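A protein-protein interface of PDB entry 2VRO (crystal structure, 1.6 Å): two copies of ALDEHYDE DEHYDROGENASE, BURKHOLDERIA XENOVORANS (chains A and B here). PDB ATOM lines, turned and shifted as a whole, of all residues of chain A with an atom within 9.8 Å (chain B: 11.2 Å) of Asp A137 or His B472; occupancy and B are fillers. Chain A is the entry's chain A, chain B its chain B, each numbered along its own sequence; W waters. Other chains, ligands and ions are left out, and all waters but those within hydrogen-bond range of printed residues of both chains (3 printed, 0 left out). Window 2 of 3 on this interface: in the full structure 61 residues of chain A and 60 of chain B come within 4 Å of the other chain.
Water W2 bridges the backbone carbonyl oxygen of Ser B473 (2.6 Å) and the backbone carbonyl oxygen of Leu A134 (2.7 Å). Water W3 lies within hydrogen-bond range of the backbone carbonyl oxygen of Ser A139 and the side-chain hydroxyl of Ser B469. Water W1 lies within hydrogen-bond range of the backbone carbonyl oxygen of Ala B465, the backbone NH of Ala A516 and the side-chain hydroxyl of Ser B467.
Among the printed residues, pairs that only touch across the chains: Ser A139 with Val B470 (3.3 Å), Phe A140 with His B464 (3.4 Å), Phe A140 with Thr B475 (3.5 Å), Ala A516 with Asp B446 (3.5 Å), Phe A140 with Ala B465 (3.5 Å), Ala A516 with Ser B469 (3.5 Å), Phe A140 with Ser B473 (3.5 Å), Ala A516 with Val B470 (3.6 Å), Ala A515 with Ala B465 (3.7 Å), Ser A135 with Ser B473 (3.7 Å), Phe A140 with Val B470 (3.8 Å), Phe A140 with Gln B474 (3.8 Å) and Leu A134 with Thr B475 (3.9 Å).
The backbone NH (N) of Arg A138 sits at hydrogen-bond distance from the side-chain hydroxyl (OG) of Ser A135 (3.3 Å). N of Ser A139 sits at hydrogen-bond distance from OG of Ser A135, 3.2 Å away. The backbone carbonyl oxygen (O) of Ser A139 sits at hydrogen-bond distance from the backbone NH (N) of Ser A517. N of Ser A141 sits at hydrogen-bond distance from O of Ala A515, 2.9 Å away. OD1 of Asp B446 lies within hydrogen-bond range of OG of Ser B467 (2.7 Å). The side-chain carboxylate (OD2) of Asp B446 sits at hydrogen-bond distance from the side-chain hydroxyl (OG) of Ser B469.
No position is printed for both chains.
Of chain B, only His B472 comes within 4 Å of Asp A137. Of chain B, only Ser B473 comes within 4 Å of Ser A135. No residue of chain A comes within 4 Å of Gln B471. Printed residues of chain A within 4 Å of Ser B473: Ser A135 (3.7 Å), Ser A139 (2.8 Å) and Phe A140 (3.5 Å). Of the printed residues of chain A, Asp B446 touches Ala A516 (3.5 Å). Of the printed residues of chain A, Val B470 touches Ser A139, Phe A140 and Ala A516. Of the printed residues of chain A, Ser B469 touches Ala A516 (3.5 Å). Of the printed residues of chain B, Ala A516 touches Asp B446 (3.5 Å), Ser B469 (3.5 Å) and Val B470 (3.6 Å). The nearest residue of chain B that does not touch Asp A137 is Ser B473 (4.2 Å).
Of the 21 printed residues of chain B, 9 touch a printed residue of chain A. Hydrophobic or aromatic side chains of chain A that line the printed part of chain B: Phe A140, Ala A515 and Ala A516. Among the printed residues, 16 pairs touch across the chains. Among the printed residues, no Asp or Glu carboxylate lies within 4 Å of a Lys or Arg side-chain nitrogen of the other chain.
The side-chain carboxylate of Asp A137 sits at hydrogen-bond distance from a ring nitrogen (NE2) of His B472 (2.5 Å). NE2 of His B472 sits close to OG of Ser A139 (3.4 Å). The side-chain hydroxyl (OG) of Ser B473 lies within hydrogen-bond range of the side-chain hydroxyl (OG) of Ser A139 (2.8 Å).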
ATOM      1  N   SER A 133     -19.500  29.909  -1.891  1.00  0.00           N
ATOM      2  CA  SER A 133     -19.196  28.805  -2.792  1.00  0.00           C
ATOM      3  C   SER A 133     -18.787  29.321  -4.174  1.00  0.00           C
ATOM      4  O   SER A 133     -19.398  30.262  -4.696  1.00  0.00           O
ATOM      5  CB  SER A 133     -20.394  27.861  -2.928  1.00  0.00           C
ATOM      6  OG  SER A 133     -20.050  26.782  -3.772  1.00  0.00           O
ATOM      7  N   LEU A 134     -17.752  28.701  -4.748  1.00  0.00           N
ATOM      8  CA  LEU A 134     -17.334  28.987  -6.125  1.00  0.00           C
ATOM      9  C   LEU A 134     -17.523  27.779  -7.063  1.00  0.00           C
ATOM     10  O   LEU A 134     -17.043  27.780  -8.198  1.00  0.00           O
ATOM     11  CB  LEU A 134     -15.871  29.468  -6.158  1.00  0.00           C
ATOM     12  CG  LEU A 134     -15.478  30.772  -5.454  1.00  0.00           C
ATOM     13  CD1 LEU A 134     -13.980  30.983  -5.533  1.00  0.00           C
ATOM     14  CD2 LEU A 134     -16.201  31.977  -6.036  1.00  0.00           C
ATOM     15  N   SER A 135     -18.240  26.757  -6.608  1.00  0.00           N
ATOM     16  CA  SER A 135     -18.467  25.575  -7.442  1.00  0.00           C
ATOM     17  C   SER A 135     -19.814  24.954  -7.129  1.00  0.00           C
ATOM     18  O   SER A 135     -20.269  25.026  -5.989  1.00  0.00           O
ATOM     19  CB  SER A 135     -17.380  24.530  -7.207  1.00  0.00           C
ATOM     20  OG  SER A 135     -17.235  24.252  -5.825  1.00  0.00           O
ATOM     21  N   LYS A 136     -20.431  24.324  -8.134  1.00  0.00           N
ATOM     22  CA  LYS A 136     -21.720  23.646  -7.925  1.00  0.00           C
ATOM     23  C   LYS A 136     -21.673  22.620  -6.787  1.00  0.00           C
ATOM     24  O   LYS A 136     -22.598  22.548  -5.974  1.00  0.00           O
ATOM     25  CB  LYS A 136     -22.249  23.001  -9.216  1.00  0.00           C
ATOM     26  CG  LYS A 136     -23.738  22.571  -9.138  1.00  0.00           C
ATOM     27  CD  LYS A 136     -24.678  23.787  -9.002  1.00  0.00           C
ATOM     28  CE  LYS A 136     -26.153  23.426  -9.230  1.00  0.00           C
ATOM     29  NZ  LYS A 136     -26.694  22.503  -8.170  1.00  0.00           N
ATOM     30  N   ASP A 137     -20.593  21.847  -6.707  1.00  0.00           N
ATOM     31  CA  ASP A 137     -20.476  20.836  -5.648  1.00  0.00           C
ATOM     32  C   ASP A 137     -19.934  21.359  -4.307  1.00  0.00           C
ATOM     33  O   ASP A 137     -19.764  20.585  -3.354  1.00  0.00           O
ATOM     34  CB  ASP A 137     -19.691  19.602  -6.129  1.00  0.00           C
ATOM     35  CG  ASP A 137     -18.202  19.882  -6.330  1.00  0.00           C
ATOM     36  OD1 ASP A 137     -17.744  21.024  -6.075  1.00  0.00           O
ATOM     37  OD2 ASP A 137     -17.487  18.937  -6.729  1.00  0.00           O
ATOM     38  N   ARG A 138     -19.647  22.665  -4.246  1.00  0.00           N
ATOM     39  CA  ARG A 138     -19.198  23.339  -3.011  1.00  0.00           C
ATOM     40  C   ARG A 138     -17.834  22.872  -2.490  1.00  0.00           C
ATOM     41  O   ARG A 138     -17.526  23.059  -1.310  1.00  0.00           O
ATOM     42  CB  ARG A 138     -20.247  23.213  -1.883  1.00  0.00           C
ATOM     43  CG  ARG A 138     -21.646  23.685  -2.237  1.00  0.00           C
ATOM     44  CD  ARG A 138     -22.601  23.411  -1.074  1.00  0.00           C
ATOM     45  NE  ARG A 138     -22.283  24.247   0.084  1.00  0.00           N
ATOM     46  CZ  ARG A 138     -22.702  25.505   0.234  1.00  0.00           C
ATOM     47  NH1 ARG A 138     -23.452  26.078  -0.703  1.00  0.00           N
ATOM     48  NH2 ARG A 138     -22.363  26.196   1.317  1.00  0.00           N
ATOM     49  N   SER A 139     -17.021  22.271  -3.359  1.00  0.00           N
ATOM     50  CA  SER A 139     -15.707  21.770  -2.971  1.00  0.00           C
ATOM     51  C   SER A 139     -14.692  22.907  -2.945  1.00  0.00           C
ATOM     52  O   SER A 139     -13.680  22.831  -2.248  1.00  0.00           O
ATOM     53  CB  SER A 139     -15.231  20.646  -3.907  1.00  0.00           C
ATOM     54  OG  SER A 139     -15.250  21.053  -5.263  1.00  0.00           O
ATOM     55  N   PHE A 140     -14.999  23.949  -3.722  1.00  0.00           N
ATOM     56  CA  PHE A 140     -14.136  25.119  -3.864  1.00  0.00           C
ATOM     57  C   PHE A 140     -14.917  26.361  -3.438  1.00  0.00           C
ATOM     58  O   PHE A 140     -16.007  26.626  -3.949  1.00  0.00           O
ATOM     59  CB  PHE A 140     -13.646  25.244  -5.318  1.00  0.00           C
ATOM     60  CG  PHE A 140     -12.502  26.204  -5.503  1.00  0.00           C
ATOM     61  CD1 PHE A 140     -11.230  25.891  -5.025  1.00  0.00           C
ATOM     62  CD2 PHE A 140     -12.688  27.419  -6.179  1.00  0.00           C
ATOM     63  CE1 PHE A 140     -10.151  26.784  -5.189  1.00  0.00           C
ATOM     64  CE2 PHE A 140     -11.614  28.313  -6.348  1.00  0.00           C
ATOM     65  CZ  PHE A 140     -10.356  27.990  -5.867  1.00  0.00           C
ATOM     66  N   SER A 141     -14.361  27.104  -2.478  1.00  0.00           N
ATOM     67  CA  SER A 141     -15.039  28.258  -1.872  1.00  0.00           C
ATOM     68  C   SER A 141     -14.082  29.426  -1.649  1.00  0.00           C
ATOM     69  O   SER A 141     -12.878  29.286  -1.821  1.00  0.00           O
ATOM     70  CB  SER A 141     -15.667  27.866  -0.529  1.00  0.00           C
ATOM     71  OG  SER A 141     -16.673  26.897  -0.741  1.00  0.00           O
ATOM     72  N   ALA A 515     -10.045  28.464  -2.078  1.00  0.00           N
ATOM     73  CA  ALA A 515      -9.451  27.190  -1.691  1.00  0.00           C
ATOM     74  C   ALA A 515     -10.505  26.098  -1.511  1.00  0.00           C
ATOM     75  O   ALA A 515     -11.714  26.378  -1.442  1.00  0.00           O
ATOM     76  CB  ALA A 515      -8.639  27.348  -0.388  1.00  0.00           C
ATOM     77  N   ALA A 516     -10.014  24.862  -1.433  1.00  0.00           N
ATOM     78  CA  ALA A 516     -10.813  23.747  -0.955  1.00  0.00           C
ATOM     79  C   ALA A 516     -11.616  24.188   0.267  1.00  0.00           C
ATOM     80  O   ALA A 516     -11.097  24.857   1.164  1.00  0.00           O
ATOM     81  CB  ALA A 516      -9.898  22.579  -0.605  1.00  0.00           C
ATOM     82  N   SER A 517     -12.884  23.806   0.301  1.00  0.00           N
ATOM     83  CA  SER A 517     -13.799  24.284   1.338  1.00  0.00           C
ATOM     84  C   SER A 517     -13.362  23.943   2.758  1.00  0.00           C
ATOM     85  O   SER A 517     -13.631  24.719   3.683  1.00  0.00           O
ATOM     86  CB  SER A 517     -15.233  23.813   1.073  1.00  0.00           C
ATOM     87  OG  SER A 517     -15.701  24.388  -0.129  1.00  0.00           O
ATOM     88  N   ALA A 518     -12.678  22.810   2.929  1.00  0.00           N
ATOM     89  CA  ALA A 518     -12.145  22.413   4.244  1.00  0.00           C
ATOM     90  C   ALA A 518     -11.199  23.481   4.785  1.00  0.00           C
ATOM     91  O   ALA A 518     -11.324  23.907   5.943  1.00  0.00           O
ATOM     92  CB  ALA A 518     -11.430  21.063   4.163  1.00  0.00           C
ATOM     93  N   PRO B 276      -0.274  13.899  -6.950  1.00  0.00           N
ATOM     94  CA  PRO B 276      -1.205  14.600  -7.839  1.00  0.00           C
ATOM     95  C   PRO B 276      -1.045  16.131  -7.858  1.00  0.00           C
ATOM     96  O   PRO B 276      -1.212  16.735  -8.926  1.00  0.00           O
ATOM     97  CB  PRO B 276      -2.585  14.198  -7.299  1.00  0.00           C
ATOM     98  CG  PRO B 276      -2.359  12.911  -6.612  1.00  0.00           C
ATOM     99  CD  PRO B 276      -0.998  13.023  -6.004  1.00  0.00           C
ATOM    100  N   LEU B 280      -0.842  19.259 -11.076  1.00  0.00           N
ATOM    101  CA  LEU B 280      -1.732  20.433 -11.059  1.00  0.00           C
ATOM    102  C   LEU B 280      -0.933  21.734 -11.183  1.00  0.00           C
ATOM    103  O   LEU B 280      -1.355  22.663 -11.887  1.00  0.00           O
ATOM    104  CB  LEU B 280      -2.582  20.438  -9.777  1.00  0.00           C
ATOM    105  CG  LEU B 280      -3.497  19.237  -9.530  1.00  0.00           C
ATOM    106  CD1 LEU B 280      -4.229  19.405  -8.208  1.00  0.00           C
ATOM    107  CD2 LEU B 280      -4.461  19.064 -10.697  1.00  0.00           C
ATOM    108  N   LYS B 283       0.431  22.065 -14.798  1.00  0.00           N
ATOM    109  CA  LYS B 283      -0.682  22.419 -15.668  1.00  0.00           C
ATOM    110  C   LYS B 283      -1.018  23.899 -15.529  1.00  0.00           C
ATOM    111  O   LYS B 283      -1.174  24.604 -16.534  1.00  0.00           O
ATOM    112  CB  LYS B 283      -1.908  21.531 -15.375  1.00  0.00           C
ATOM    113  CG  LYS B 283      -1.804  20.121 -15.966  1.00  0.00           C
ATOM    114  CD  LYS B 283      -2.933  19.233 -15.427  1.00  0.00           C
ATOM    115  CE  LYS B 283      -2.679  17.755 -15.724  1.00  0.00           C
ATOM    116  NZ  LYS B 283      -3.529  17.247 -16.844  1.00  0.00           N
ATOM    117  N   GLU B 284      -1.079  24.381 -14.292  1.00  0.00           N
ATOM    118  CA  GLU B 284      -1.485  25.772 -14.028  1.00  0.00           C
ATOM    119  C   GLU B 284      -0.446  26.787 -14.523  1.00  0.00           C
ATOM    120  O   GLU B 284      -0.803  27.828 -15.121  1.00  0.00           O
ATOM    121  CB  GLU B 284      -1.817  25.983 -12.539  1.00  0.00           C
ATOM    122  CG  GLU B 284      -2.798  27.129 -12.323  1.00  0.00           C
ATOM    123  CD  GLU B 284      -4.226  26.802 -12.766  1.00  0.00           C
ATOM    124  OE1 GLU B 284      -4.511  25.609 -13.080  1.00  0.00           O
ATOM    125  OE2 GLU B 284      -5.061  27.744 -12.795  1.00  0.00           O
ATOM    126  N   ARG B 287      -0.778  26.932 -18.399  1.00  0.00           N
ATOM    127  CA  ARG B 287      -2.021  27.649 -18.735  1.00  0.00           C
ATOM    128  C   ARG B 287      -1.839  29.173 -18.627  1.00  0.00           C
ATOM    129  O   ARG B 287      -2.209  29.936 -19.538  1.00  0.00           O
ATOM    130  CB  ARG B 287      -3.175  27.187 -17.834  1.00  0.00           C
ATOM    131  CG  ARG B 287      -4.566  27.540 -18.364  1.00  0.00           C
ATOM    132  CD  ARG B 287      -5.585  26.431 -18.034  1.00  0.00           C
ATOM    133  NE  ARG B 287      -6.017  26.431 -16.634  1.00  0.00           N
ATOM    134  CZ  ARG B 287      -6.341  25.339 -15.932  1.00  0.00           C
ATOM    135  NH1 ARG B 287      -6.271  24.127 -16.482  1.00  0.00           N
ATOM    136  NH2 ARG B 287      -6.728  25.459 -14.668  1.00  0.00           N
ATOM    137  N   ASP B 446      -5.082  19.671   2.087  1.00  0.00           N
ATOM    138  CA  ASP B 446      -6.031  20.790   2.288  1.00  0.00           C
ATOM    139  C   ASP B 446      -5.896  21.480   3.659  1.00  0.00           C
ATOM    140  O   ASP B 446      -6.162  22.673   3.767  1.00  0.00           O
ATOM    141  CB  ASP B 446      -7.490  20.353   2.078  1.00  0.00           C
ATOM    142  CG  ASP B 446      -7.804  19.936   0.629  1.00  0.00           C
ATOM    143  OD1 ASP B 446      -6.976  20.154  -0.286  1.00  0.00           O
ATOM    144  OD2 ASP B 446      -8.909  19.377   0.407  1.00  0.00           O
ATOM    145  N   HIS B 464      -4.885  31.850  -4.197  1.00  0.00           N
ATOM    146  CA  HIS B 464      -5.654  30.850  -4.924  1.00  0.00           C
ATOM    147  C   HIS B 464      -5.012  29.480  -4.679  1.00  0.00           C
ATOM    148  O   HIS B 464      -3.921  29.210  -5.176  1.00  0.00           O
ATOM    149  CB  HIS B 464      -5.637  31.170  -6.416  1.00  0.00           C
ATOM    150  CG  HIS B 464      -6.607  30.359  -7.204  1.00  0.00           C
ATOM    151  ND1 HIS B 464      -6.239  29.255  -7.939  1.00  0.00           N
ATOM    152  CD2 HIS B 464      -7.947  30.484  -7.350  1.00  0.00           C
ATOM    153  CE1 HIS B 464      -7.310  28.754  -8.530  1.00  0.00           C
ATOM    154  NE2 HIS B 464      -8.361  29.470  -8.169  1.00  0.00           N
ATOM    155  N   ALA B 465      -5.678  28.629  -3.901  1.00  0.00           N
ATOM    156  CA  ALA B 465      -5.074  27.349  -3.496  1.00  0.00           C
ATOM    157  C   ALA B 465      -5.612  26.211  -4.353  1.00  0.00           C
ATOM    158  O   ALA B 465      -6.822  25.994  -4.439  1.00  0.00           O
ATOM    159  CB  ALA B 465      -5.313  27.071  -2.005  1.00  0.00           C
ATOM    160  N   ILE B 466      -4.688  25.499  -4.988  1.00  0.00           N
ATOM    161  CA  ILE B 466      -5.001  24.364  -5.839  1.00  0.00           C
ATOM    162  C   ILE B 466      -4.517  23.053  -5.212  1.00  0.00           C
ATOM    163  O   ILE B 466      -3.355  22.912  -4.841  1.00  0.00           O
ATOM    164  CB  ILE B 466      -4.365  24.556  -7.254  1.00  0.00           C
ATOM    165  CG1 ILE B 466      -4.930  25.812  -7.929  1.00  0.00           C
ATOM    166  CG2 ILE B 466      -4.563  23.329  -8.134  1.00  0.00           C
ATOM    167  CD1 ILE B 466      -6.354  26.031  -7.691  1.00  0.00           C
ATOM    168  N   SER B 467      -5.440  22.099  -5.093  1.00  0.00           N
ATOM    169  CA  SER B 467      -5.153  20.797  -4.496  1.00  0.00           C
ATOM    170  C   SER B 467      -6.051  19.753  -5.178  1.00  0.00           C
ATOM    171  O   SER B 467      -7.054  20.113  -5.790  1.00  0.00           O
ATOM    172  CB  SER B 467      -5.413  20.840  -2.978  1.00  0.00           C
ATOM    173  OG  SER B 467      -6.738  21.272  -2.698  1.00  0.00           O
ATOM    174  N   PRO B 468      -5.697  18.451  -5.058  1.00  0.00           N
ATOM    175  CA  PRO B 468      -6.462  17.365  -5.679  1.00  0.00           C
ATOM    176  C   PRO B 468      -7.976  17.448  -5.471  1.00  0.00           C
ATOM    177  O   PRO B 468      -8.717  17.249  -6.431  1.00  0.00           O
ATOM    178  CB  PRO B 468      -5.882  16.112  -5.024  1.00  0.00           C
ATOM    179  CG  PRO B 468      -4.433  16.482  -4.814  1.00  0.00           C
ATOM    180  CD  PRO B 468      -4.508  17.936  -4.352  1.00  0.00           C
ATOM    181  N   SER B 469      -8.428  17.768  -4.255  1.00  0.00           N
ATOM    182  CA  SER B 469      -9.870  17.811  -3.975  1.00  0.00           C
ATOM    183  C   SER B 469     -10.606  18.854  -4.815  1.00  0.00           C
ATOM    184  O   SER B 469     -11.832  18.789  -4.949  1.00  0.00           O
ATOM    185  CB  SER B 469     -10.171  18.033  -2.482  1.00  0.00           C
ATOM    186  OG  SER B 469      -9.971  19.379  -2.077  1.00  0.00           O
ATOM    187  N   VAL B 470      -9.856  19.816  -5.359  1.00  0.00           N
ATOM    188  CA  VAL B 470     -10.461  20.850  -6.202  1.00  0.00           C
ATOM    189  C   VAL B 470      -9.920  20.856  -7.633  1.00  0.00           C
ATOM    190  O   VAL B 470     -10.064  21.850  -8.342  1.00  0.00           O
ATOM    191  CB  VAL B 470     -10.405  22.268  -5.545  1.00  0.00           C
ATOM    192  CG1 VAL B 470     -11.095  22.233  -4.187  1.00  0.00           C
ATOM    193  CG2 VAL B 470      -8.959  22.757  -5.379  1.00  0.00           C
ATOM    194  N   GLN B 471      -9.350  19.730  -8.074  1.00  0.00           N
ATOM    195  CA  GLN B 471      -8.835  19.641  -9.451  1.00  0.00           C
ATOM    196  C   GLN B 471      -9.877  20.017 -10.521  1.00  0.00           C
ATOM    197  O   GLN B 471      -9.560  20.663 -11.517  1.00  0.00           O
ATOM    198  CB  GLN B 471      -8.246  18.249  -9.730  1.00  0.00           C
ATOM    199  CG  GLN B 471      -9.234  17.089  -9.682  1.00  0.00           C
ATOM    200  CD  GLN B 471      -8.665  15.817 -10.315  1.00  0.00           C
ATOM    201  OE1 GLN B 471      -7.488  15.762 -10.687  1.00  0.00           O
ATOM    202  NE2 GLN B 471      -9.510  14.798 -10.453  1.00  0.00           N
ATOM    203  N   HIS B 472     -11.123  19.631 -10.273  1.00  0.00           N
ATOM    204  CA  HIS B 472     -12.247  19.815 -11.202  1.00  0.00           C
ATOM    205  C   HIS B 472     -13.025  21.123 -10.960  1.00  0.00           C
ATOM    206  O   HIS B 472     -13.825  21.561 -11.806  1.00  0.00           O
ATOM    207  CB  HIS B 472     -13.215  18.651 -10.979  1.00  0.00           C
ATOM    208  CG  HIS B 472     -13.885  18.699  -9.639  1.00  0.00           C
ATOM    209  ND1 HIS B 472     -13.186  18.597  -8.449  1.00  0.00           N
ATOM    210  CD2 HIS B 472     -15.184  18.885  -9.299  1.00  0.00           C
ATOM    211  CE1 HIS B 472     -14.032  18.696  -7.441  1.00  0.00           C
ATOM    212  NE2 HIS B 472     -15.249  18.873  -7.929  1.00  0.00           N
ATOM    213  N   SER B 473     -12.812  21.732  -9.797  1.00  0.00           N
ATOM    214  CA  SER B 473     -13.651  22.848  -9.372  1.00  0.00           C
ATOM    215  C   SER B 473     -12.920  24.169  -9.211  1.00  0.00           C
ATOM    216  O   SER B 473     -13.551  25.207  -9.234  1.00  0.00           O
ATOM    217  CB  SER B 473     -14.361  22.527  -8.058  1.00  0.00           C
ATOM    218  OG  SER B 473     -13.426  22.186  -7.059  1.00  0.00           O
ATOM    219  N   GLN B 474     -11.602  24.125  -9.010  1.00  0.00           N
ATOM    220  CA  GLN B 474     -10.827  25.349  -8.846  1.00  0.00           C
ATOM    221  C   GLN B 474     -10.975  26.215 -10.106  1.00  0.00           C
ATOM    222  O   GLN B 474     -10.949  25.706 -11.226  1.00  0.00           O
ATOM    223  CB  GLN B 474      -9.358  25.021  -8.552  1.00  0.00           C
ATOM    224  CG  GLN B 474      -8.605  24.385  -9.718  1.00  0.00           C
ATOM    225  CD  GLN B 474      -7.766  25.392 -10.506  1.00  0.00           C
ATOM    226  OE1 GLN B 474      -7.896  26.600 -10.321  1.00  0.00           O
ATOM    227  NE2 GLN B 474      -6.873  24.883 -11.363  1.00  0.00           N
ATOM    228  N   THR B 475     -11.140  27.520  -9.897  1.00  0.00           N
ATOM    229  CA  THR B 475     -11.548  28.448 -10.964  1.00  0.00           C
ATOM    230  C   THR B 475     -10.382  29.101 -11.727  1.00  0.00           C
ATOM    231  O   THR B 475     -10.606  30.014 -12.517  1.00  0.00           O
ATOM    232  CB  THR B 475     -12.414  29.568 -10.378  1.00  0.00           C
ATOM    233  OG1 THR B 475     -11.711  30.147  -9.272  1.00  0.00           O
ATOM    234  CG2 THR B 475     -13.813  29.011  -9.921  1.00  0.00           C
ATOM    235  N   GLY B 476      -9.154  28.649 -11.495  1.00  0.00           N
ATOM    236  CA  GLY B 476      -8.001  29.166 -12.261  1.00  0.00           C
ATOM    237  C   GLY B 476      -7.226  30.230 -11.526  1.00  0.00           C
ATOM    238  O   GLY B 476      -7.812  31.141 -10.914  1.00  0.00           O
ATOM    239  N   ASN B 479      -7.895  33.656 -13.584  1.00  0.00           N
ATOM    240  CA  ASN B 479      -9.295  34.036 -13.824  1.00  0.00           C
ATOM    241  C   ASN B 479      -9.879  34.776 -12.648  1.00  0.00           C
ATOM    242  O   ASN B 479      -9.727  34.364 -11.492  1.00  0.00           O
ATOM    243  CB  ASN B 479     -10.143  32.808 -14.149  1.00  0.00           C
ATOM    244  CG  ASN B 479      -9.669  32.111 -15.389  1.00  0.00           C
ATOM    245  OD1 ASN B 479      -9.455  32.747 -16.426  1.00  0.00           O
ATOM    246  ND2 ASN B 479      -9.486  30.790 -15.298  1.00  0.00           N
ATOM    247  N   MET B 481     -12.834  35.771 -10.679  1.00  0.00           N
ATOM    248  CA  MET B 481     -14.224  35.497 -10.330  1.00  0.00           C
ATOM    249  C   MET B 481     -14.801  36.780  -9.710  1.00  0.00           C
ATOM    250  O   MET B 481     -14.236  37.295  -8.743  1.00  0.00           O
ATOM    251  CB  MET B 481     -14.319  34.294  -9.380  1.00  0.00           C
ATOM    252  CG  MET B 481     -13.836  32.972  -9.997  1.00  0.00           C
ATOM    253  SD  MET B 481     -14.674  32.504 -11.523  1.00  0.00           S
ATOM    254  CE  MET B 481     -13.478  33.038 -12.741  1.00  0.00           C
HETATM  255  O   HOH W   1      -7.405  24.167  -2.375  1.00  0.00           O
HETATM  256  O   HOH W   2     -15.982  25.920  -9.877  1.00  0.00           O
HETATM  257  O   HOH W   3     -12.571  20.379  -1.419  1.00  0.00           O
